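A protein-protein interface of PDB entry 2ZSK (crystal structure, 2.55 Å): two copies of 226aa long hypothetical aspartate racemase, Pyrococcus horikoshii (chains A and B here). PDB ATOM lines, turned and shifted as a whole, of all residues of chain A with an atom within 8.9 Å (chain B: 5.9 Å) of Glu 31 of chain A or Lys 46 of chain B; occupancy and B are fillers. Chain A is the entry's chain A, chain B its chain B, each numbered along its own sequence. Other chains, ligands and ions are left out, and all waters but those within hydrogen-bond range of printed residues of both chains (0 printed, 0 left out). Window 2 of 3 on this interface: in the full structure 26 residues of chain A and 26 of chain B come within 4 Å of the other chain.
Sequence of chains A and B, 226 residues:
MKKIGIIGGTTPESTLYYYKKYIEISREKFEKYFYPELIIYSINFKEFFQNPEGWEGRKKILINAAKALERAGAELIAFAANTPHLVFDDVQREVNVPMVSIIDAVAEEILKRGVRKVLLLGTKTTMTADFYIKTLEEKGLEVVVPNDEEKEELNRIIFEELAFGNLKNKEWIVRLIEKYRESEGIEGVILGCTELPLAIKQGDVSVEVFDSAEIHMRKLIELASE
Printed residues of chain B that touch a printed residue of chain A: Asn 44, Phe 45, Lys 46, Phe 49 and Gln 50. Printed residues of chain A that touch a printed residue of chain B: Glu 31, Lys 32, Tyr 33, Phe 34 and Tyr 35. Hydrophobic or aromatic side chains of chain A within 4 Å of the printed part of chain B: Tyr 33 and Phe 34. Among the printed residues, 10 pairs touch across the chains. Among the printed residues, Asp or Glu carboxylates within 4 Å of a Lys or Arg side-chain nitrogen of the other chain: Glu 31 of chain A with Lys 46 of chain B.
N of Lys 46 of chain B lies close to OD1 of Asn 44 of chain B (3.4 Å). The guanidinium group of Arg 27 of chain A lies within hydrogen-bond range of the side-chain hydroxyl of Tyr 35 of chain A. OE1 of Gln 50 of chain B sits at hydrogen-bond distance from NZ of Lys 46 of chain B (3.0 Å). The side-chain amide nitrogen (ND2) of Asn 44 of chain B is in hydrogen-bond range of the side-chain carboxylate (OE2) of Glu 47 of chain B (3.2 Å).
O of Tyr 33 of chain A touches OD1 of Asn 44 of chain B (3.9 Å). O of Tyr 33 of chain A touches CB of Phe 45 of chain B, 3.2 Å away. Tyr 33 of chain A touches Phe 49 of chain B (CZ to CE2, 3.5 Å). Tyr 33 of chain A touches Gln 50 of chain B. Asn 44 of chain B touches Phe 34 of chain A. Phe 34 of chain A touches Lys 46 of chain B (N to CB, 3.8 Å).
No position is printed for both chains.
OE2 of Glu 31 of chain A lies within salt-bridge range of NZ of Lys 46 of chain B (3.7 Å). O of Tyr 33 of chain A lies within hydrogen-bond range of N of Lys 46 of chain B, at 2.8 Å. O of Lys 32 of chain A sits at hydrogen-bond distance from NZ of Lys 46 of chain B, 2.9 Å away. OD1 of Asn 44 of chain B sits at hydrogen-bond distance from N of Tyr 35 of chain A, 3.1 Å away.
Of chain B, only Lys 46 comes within 4 Å of Glu 31 of chain A. Printed residues of chain B within 4 Å of Phe 34 of chain A: Asn 44 and Lys 46. Printed residues of chain B within 4 Å of Tyr 35 of chain A: Asn 44. Lys 46 of chain B touches four residues of chain A. Of the printed residues of chain A, Phe 49 of chain B touches Tyr 33 (3.5 Å). Printed residues of chain A within 4 Å of Gln 50 of chain B: Tyr 33 (3.6 Å). The nearest printed residue of chain B that does not touch Glu 31 of chain A is Gln 50 of chain B (6.2 Å). The nearest printed residue of chain B that does not touch Lys 32 of chain A is Gln 50 of chain B (4.9 Å).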
ATOM      1  N   ILE A  23      25.632  -8.880  15.689  1.00  0.00           N
ATOM      2  CA  ILE A  23      25.801  -8.332  14.350  1.00  0.00           C
ATOM      3  C   ILE A  23      27.220  -7.786  14.197  1.00  0.00           C
ATOM      4  O   ILE A  23      27.924  -8.133  13.247  1.00  0.00           O
ATOM      5  CB  ILE A  23      24.765  -7.218  14.068  1.00  0.00           C
ATOM      6  CG1 ILE A  23      23.355  -7.821  14.031  1.00  0.00           C
ATOM      7  CG2 ILE A  23      25.065  -6.543  12.749  1.00  0.00           C
ATOM      8  CD1 ILE A  23      22.245  -6.797  14.135  1.00  0.00           C
ATOM      9  N   ILE A  25      30.075  -8.360  15.982  1.00  0.00           N
ATOM     10  CA  ILE A  25      31.058  -9.435  16.046  1.00  0.00           C
ATOM     11  C   ILE A  25      31.140 -10.268  14.774  1.00  0.00           C
ATOM     12  O   ILE A  25      32.236 -10.634  14.352  1.00  0.00           O
ATOM     13  CB  ILE A  25      30.770 -10.350  17.251  1.00  0.00           C
ATOM     14  CG1 ILE A  25      30.852  -9.514  18.539  1.00  0.00           C
ATOM     15  CG2 ILE A  25      31.749 -11.534  17.262  1.00  0.00           C
ATOM     16  CD1 ILE A  25      30.451 -10.233  19.815  1.00  0.00           C
ATOM     17  N   SER A  26      29.990 -10.550  14.163  1.00  0.00           N
ATOM     18  CA  SER A  26      29.943 -11.339  12.931  1.00  0.00           C
ATOM     19  C   SER A  26      30.611 -10.614  11.760  1.00  0.00           C
ATOM     20  O   SER A  26      31.421 -11.199  11.036  1.00  0.00           O
ATOM     21  CB  SER A  26      28.492 -11.671  12.552  1.00  0.00           C
ATOM     22  OG  SER A  26      27.897 -12.584  13.458  1.00  0.00           O
ATOM     23  N   ARG A  27      30.269  -9.345  11.565  1.00  0.00           N
ATOM     24  CA  ARG A  27      30.856  -8.573  10.472  1.00  0.00           C
ATOM     25  C   ARG A  27      32.369  -8.500  10.633  1.00  0.00           C
ATOM     26  O   ARG A  27      33.128  -8.440   9.659  1.00  0.00           O
ATOM     27  CB  ARG A  27      30.271  -7.158  10.451  1.00  0.00           C
ATOM     28  CG  ARG A  27      28.813  -7.105  10.041  1.00  0.00           C
ATOM     29  CD  ARG A  27      28.218  -5.757  10.356  1.00  0.00           C
ATOM     30  NE  ARG A  27      26.836  -5.640   9.891  1.00  0.00           N
ATOM     31  CZ  ARG A  27      26.054  -4.592  10.140  1.00  0.00           C
ATOM     32  NH1 ARG A  27      26.522  -3.566  10.853  1.00  0.00           N
ATOM     33  NH2 ARG A  27      24.806  -4.567   9.677  1.00  0.00           N
ATOM     34  N   GLU A  28      32.794  -8.528  11.885  1.00  0.00           N
ATOM     35  CA  GLU A  28      34.192  -8.446  12.233  1.00  0.00           C
ATOM     36  C   GLU A  28      34.964  -9.750  12.120  1.00  0.00           C
ATOM     37  O   GLU A  28      36.164  -9.755  11.843  1.00  0.00           O
ATOM     38  CB  GLU A  28      34.309  -7.942  13.657  1.00  0.00           C
ATOM     39  CG  GLU A  28      35.709  -7.874  14.133  1.00  0.00           C
ATOM     40  CD  GLU A  28      35.789  -7.961  15.628  1.00  0.00           C
ATOM     41  OE1 GLU A  28      35.236  -7.064  16.302  1.00  0.00           O
ATOM     42  OE2 GLU A  28      36.401  -8.933  16.124  1.00  0.00           O
ATOM     43  N   LYS A  29      34.278 -10.860  12.329  1.00  0.00           N
ATOM     44  CA  LYS A  29      34.951 -12.140  12.308  1.00  0.00           C
ATOM     45  C   LYS A  29      34.868 -12.911  10.985  1.00  0.00           C
ATOM     46  O   LYS A  29      35.842 -13.549  10.583  1.00  0.00           O
ATOM     47  CB  LYS A  29      34.417 -12.984  13.471  1.00  0.00           C
ATOM     48  CG  LYS A  29      35.303 -14.133  13.911  1.00  0.00           C
ATOM     49  CD  LYS A  29      34.759 -14.774  15.189  1.00  0.00           C
ATOM     50  CE  LYS A  29      35.671 -15.887  15.696  1.00  0.00           C
ATOM     51  NZ  LYS A  29      35.907 -16.947  14.656  1.00  0.00           N
ATOM     52  N   PHE A  30      33.737 -12.834  10.287  1.00  0.00           N
ATOM     53  CA  PHE A  30      33.595 -13.590   9.046  1.00  0.00           C
ATOM     54  C   PHE A  30      33.521 -12.782   7.759  1.00  0.00           C
ATOM     55  O   PHE A  30      33.752 -11.577   7.751  1.00  0.00           O
ATOM     56  CB  PHE A  30      32.366 -14.501   9.135  1.00  0.00           C
ATOM     57  CG  PHE A  30      32.135 -15.077  10.505  1.00  0.00           C
ATOM     58  CD1 PHE A  30      31.307 -14.424  11.417  1.00  0.00           C
ATOM     59  CD2 PHE A  30      32.751 -16.261  10.890  1.00  0.00           C
ATOM     60  CE1 PHE A  30      31.095 -14.942  12.692  1.00  0.00           C
ATOM     61  CE2 PHE A  30      32.545 -16.785  12.165  1.00  0.00           C
ATOM     62  CZ  PHE A  30      31.712 -16.122  13.068  1.00  0.00           C
ATOM     63  N   GLU A  31      33.214 -13.474   6.664  1.00  0.00           N
ATOM     64  CA  GLU A  31      33.085 -12.849   5.353  1.00  0.00           C
ATOM     65  C   GLU A  31      31.847 -11.969   5.340  1.00  0.00           C
ATOM     66  O   GLU A  31      31.146 -11.860   6.346  1.00  0.00           O
ATOM     67  CB  GLU A  31      32.960 -13.915   4.265  1.00  0.00           C
ATOM     68  CG  GLU A  31      34.170 -14.831   4.134  1.00  0.00           C
ATOM     69  CD  GLU A  31      33.871 -16.097   3.315  1.00  0.00           C
ATOM     70  OE1 GLU A  31      34.810 -16.895   3.084  1.00  0.00           O
ATOM     71  OE2 GLU A  31      32.702 -16.299   2.908  1.00  0.00           O
ATOM     72  N   LYS A  32      31.575 -11.341   4.202  1.00  0.00           N
ATOM     73  CA  LYS A  32      30.415 -10.463   4.087  1.00  0.00           C
ATOM     74  C   LYS A  32      29.110 -11.248   4.027  1.00  0.00           C
ATOM     75  O   LYS A  32      29.033 -12.314   3.404  1.00  0.00           O
ATOM     76  CB  LYS A  32      30.550  -9.562   2.858  1.00  0.00           C
ATOM     77  N   TYR A  33      28.100 -10.703   4.700  1.00  0.00           N
ATOM     78  CA  TYR A  33      26.763 -11.281   4.760  1.00  0.00           C
ATOM     79  C   TYR A  33      26.665 -12.487   5.682  1.00  0.00           C
ATOM     80  O   TYR A  33      25.565 -12.972   5.948  1.00  0.00           O
ATOM     81  CB  TYR A  33      26.299 -11.676   3.351  1.00  0.00           C
ATOM     82  CG  TYR A  33      26.240 -10.525   2.364  1.00  0.00           C
ATOM     83  CD1 TYR A  33      26.714 -10.682   1.055  1.00  0.00           C
ATOM     84  CD2 TYR A  33      25.687  -9.293   2.726  1.00  0.00           C
ATOM     85  CE1 TYR A  33      26.633  -9.645   0.133  1.00  0.00           C
ATOM     86  CE2 TYR A  33      25.601  -8.248   1.810  1.00  0.00           C
ATOM     87  CZ  TYR A  33      26.074  -8.428   0.515  1.00  0.00           C
ATOM     88  OH  TYR A  33      25.972  -7.399  -0.400  1.00  0.00           O
ATOM     89  N   PHE A  34      27.810 -12.953   6.183  1.00  0.00           N
ATOM     90  CA  PHE A  34      27.853 -14.135   7.048  1.00  0.00           C
ATOM     91  C   PHE A  34      27.524 -13.908   8.518  1.00  0.00           C
ATOM     92  O   PHE A  34      28.199 -13.148   9.218  1.00  0.00           O
ATOM     93  CB  PHE A  34      29.222 -14.813   6.965  1.00  0.00           C
ATOM     94  CG  PHE A  34      29.248 -16.194   7.553  1.00  0.00           C
ATOM     95  CD1 PHE A  34      29.064 -17.309   6.740  1.00  0.00           C
ATOM     96  CD2 PHE A  34      29.434 -16.385   8.925  1.00  0.00           C
ATOM     97  CE1 PHE A  34      29.069 -18.606   7.277  1.00  0.00           C
ATOM     98  CE2 PHE A  34      29.442 -17.673   9.479  1.00  0.00           C
ATOM     99  CZ  PHE A  34      29.255 -18.790   8.643  1.00  0.00           C
ATOM    100  N   TYR A  35      26.478 -14.591   8.975  1.00  0.00           N
ATOM    101  CA  TYR A  35      26.045 -14.526  10.366  1.00  0.00           C
ATOM    102  C   TYR A  35      25.653 -15.932  10.800  1.00  0.00           C
ATOM    103  O   TYR A  35      24.716 -16.516  10.264  1.00  0.00           O
ATOM    104  CB  TYR A  35      24.848 -13.612  10.527  1.00  0.00           C
ATOM    105  CG  TYR A  35      25.102 -12.184  10.131  1.00  0.00           C
ATOM    106  CD1 TYR A  35      25.005 -11.781   8.803  1.00  0.00           C
ATOM    107  CD2 TYR A  35      25.423 -11.227  11.092  1.00  0.00           C
ATOM    108  CE1 TYR A  35      25.217 -10.459   8.442  1.00  0.00           C
ATOM    109  CE2 TYR A  35      25.639  -9.903  10.745  1.00  0.00           C
ATOM    110  CZ  TYR A  35      25.534  -9.525   9.414  1.00  0.00           C
ATOM    111  OH  TYR A  35      25.755  -8.212   9.067  1.00  0.00           O
ATOM    112  N   PRO A  36      26.363 -16.488  11.792  1.00  0.00           N
ATOM    113  CA  PRO A  36      26.062 -17.840  12.272  1.00  0.00           C
ATOM    114  C   PRO A  36      24.643 -17.962  12.848  1.00  0.00           C
ATOM    115  O   PRO A  36      24.221 -17.150  13.675  1.00  0.00           O
ATOM    116  CB  PRO A  36      27.155 -18.076  13.308  1.00  0.00           C
ATOM    117  CG  PRO A  36      27.371 -16.704  13.876  1.00  0.00           C
ATOM    118  CD  PRO A  36      27.361 -15.827  12.655  1.00  0.00           C
ATOM    119  N   ASN B  44      21.462 -17.467   8.481  1.00  0.00           N
ATOM    120  CA  ASN B  44      22.756 -17.011   7.982  1.00  0.00           C
ATOM    121  C   ASN B  44      22.469 -16.303   6.666  1.00  0.00           C
ATOM    122  O   ASN B  44      22.283 -16.956   5.631  1.00  0.00           O
ATOM    123  CB  ASN B  44      23.672 -18.206   7.717  1.00  0.00           C
ATOM    124  CG  ASN B  44      25.111 -17.800   7.481  1.00  0.00           C
ATOM    125  OD1 ASN B  44      25.390 -16.701   7.010  1.00  0.00           O
ATOM    126  ND2 ASN B  44      26.033 -18.696   7.802  1.00  0.00           N
ATOM    127  N   PHE B  45      22.432 -14.974   6.713  1.00  0.00           N
ATOM    128  CA  PHE B  45      22.129 -14.156   5.539  1.00  0.00           C
ATOM    129  C   PHE B  45      22.903 -14.506   4.275  1.00  0.00           C
ATOM    130  O   PHE B  45      22.342 -14.460   3.185  1.00  0.00           O
ATOM    131  CB  PHE B  45      22.342 -12.679   5.867  1.00  0.00           C
ATOM    132  CG  PHE B  45      21.885 -11.737   4.781  1.00  0.00           C
ATOM    133  CD1 PHE B  45      20.606 -11.845   4.242  1.00  0.00           C
ATOM    134  CD2 PHE B  45      22.718 -10.718   4.325  1.00  0.00           C
ATOM    135  CE1 PHE B  45      20.170 -10.948   3.266  1.00  0.00           C
ATOM    136  CE2 PHE B  45      22.288  -9.824   3.354  1.00  0.00           C
ATOM    137  CZ  PHE B  45      21.019  -9.933   2.825  1.00  0.00           C
ATOM    138  N   LYS B  46      24.182 -14.851   4.415  1.00  0.00           N
ATOM    139  CA  LYS B  46      24.993 -15.198   3.256  1.00  0.00           C
ATOM    140  C   LYS B  46      24.452 -16.417   2.504  1.00  0.00           C
ATOM    141  O   LYS B  46      24.483 -16.460   1.277  1.00  0.00           O
ATOM    142  CB  LYS B  46      26.439 -15.451   3.677  1.00  0.00           C
ATOM    143  CG  LYS B  46      27.382 -15.690   2.505  1.00  0.00           C
ATOM    144  CD  LYS B  46      28.771 -16.060   2.983  1.00  0.00           C
ATOM    145  CE  LYS B  46      29.791 -15.818   1.892  1.00  0.00           C
ATOM    146  NZ  LYS B  46      29.850 -14.364   1.543  1.00  0.00           N
ATOM    147  N   GLU B  47      23.964 -17.412   3.234  1.00  0.00           N
ATOM    148  CA  GLU B  47      23.414 -18.598   2.593  1.00  0.00           C
ATOM    149  C   GLU B  47      22.096 -18.253   1.890  1.00  0.00           C
ATOM    150  O   GLU B  47      21.696 -18.915   0.932  1.00  0.00           O
ATOM    151  CB  GLU B  47      23.168 -19.695   3.623  1.00  0.00           C
ATOM    152  CG  GLU B  47      24.416 -20.393   4.129  1.00  0.00           C
ATOM    153  CD  GLU B  47      24.107 -21.272   5.325  1.00  0.00           C
ATOM    154  OE1 GLU B  47      23.038 -21.923   5.314  1.00  0.00           O
ATOM    155  OE2 GLU B  47      24.924 -21.315   6.268  1.00  0.00           O
ATOM    156  N   PHE B  48      21.429 -17.211   2.373  1.00  0.00           N
ATOM    157  CA  PHE B  48      20.165 -16.760   1.809  1.00  0.00           C
ATOM    158  C   PHE B  48      20.412 -15.844   0.626  1.00  0.00           C
ATOM    159  O   PHE B  48      20.032 -16.144  -0.498  1.00  0.00           O
ATOM    160  CB  PHE B  48      19.374 -15.985   2.859  1.00  0.00           C
ATOM    161  CG  PHE B  48      18.001 -15.559   2.409  1.00  0.00           C
ATOM    162  CD1 PHE B  48      16.932 -16.441   2.475  1.00  0.00           C
ATOM    163  CD2 PHE B  48      17.766 -14.258   1.971  1.00  0.00           C
ATOM    164  CE1 PHE B  48      15.647 -16.033   2.121  1.00  0.00           C
ATOM    165  CE2 PHE B  48      16.481 -13.839   1.611  1.00  0.00           C
ATOM    166  CZ  PHE B  48      15.426 -14.726   1.689  1.00  0.00           C
ATOM    167  N   PHE B  49      21.054 -14.718   0.907  1.00  0.00           N
ATOM    168  CA  PHE B  49      21.349 -13.699  -0.091  1.00  0.00           C
ATOM    169  C   PHE B  49      22.091 -14.206  -1.329  1.00  0.00           C
ATOM    170  O   PHE B  49      21.704 -13.893  -2.448  1.00  0.00           O
ATOM    171  CB  PHE B  49      22.141 -12.564   0.565  1.00  0.00           C
ATOM    172  CG  PHE B  49      22.195 -11.311  -0.252  1.00  0.00           C
ATOM    173  CD1 PHE B  49      21.026 -10.612  -0.554  1.00  0.00           C
ATOM    174  CD2 PHE B  49      23.416 -10.812  -0.702  1.00  0.00           C
ATOM    175  CE1 PHE B  49      21.071  -9.430  -1.292  1.00  0.00           C
ATOM    176  CE2 PHE B  49      23.475  -9.635  -1.438  1.00  0.00           C
ATOM    177  CZ  PHE B  49      22.297  -8.940  -1.734  1.00  0.00           C
ATOM    178  N   GLN B  50      23.157 -14.976  -1.124  1.00  0.00           N
ATOM    179  CA  GLN B  50      23.939 -15.516  -2.233  1.00  0.00           C
ATOM    180  C   GLN B  50      23.689 -17.016  -2.321  1.00  0.00           C
ATOM    181  O   GLN B  50      24.620 -17.817  -2.190  1.00  0.00           O
ATOM    182  CB  GLN B  50      25.436 -15.294  -2.006  1.00  0.00           C
ATOM    183  CG  GLN B  50      25.801 -13.929  -1.482  1.00  0.00           C
ATOM    184  CD  GLN B  50      27.295 -13.773  -1.268  1.00  0.00           C
ATOM    185  OE1 GLN B  50      27.949 -14.656  -0.707  1.00  0.00           O
ATOM    186  NE2 GLN B  50      27.843 -12.637  -1.705  1.00  0.00           N
ATOM    187  N   ASN B  51      22.430 -17.402  -2.517  1.00  0.00           N
ATOM    188  CA  ASN B  51      22.094 -18.816  -2.623  1.00  0.00           C
ATOM    189  C   ASN B  51      22.305 -19.266  -4.061  1.00  0.00           C
ATOM    190  O   ASN B  51      21.796 -18.662  -4.996  1.00  0.00           O
ATOM    191  CB  ASN B  51      20.643 -19.068  -2.202  1.00  0.00           C
ATOM    192  CG  ASN B  51      20.380 -20.528  -1.869  1.00  0.00           C
ATOM    193  OD1 ASN B  51      20.359 -21.386  -2.752  1.00  0.00           O
ATOM    194  ND2 ASN B  51      20.199 -20.818  -0.584  1.00  0.00           N
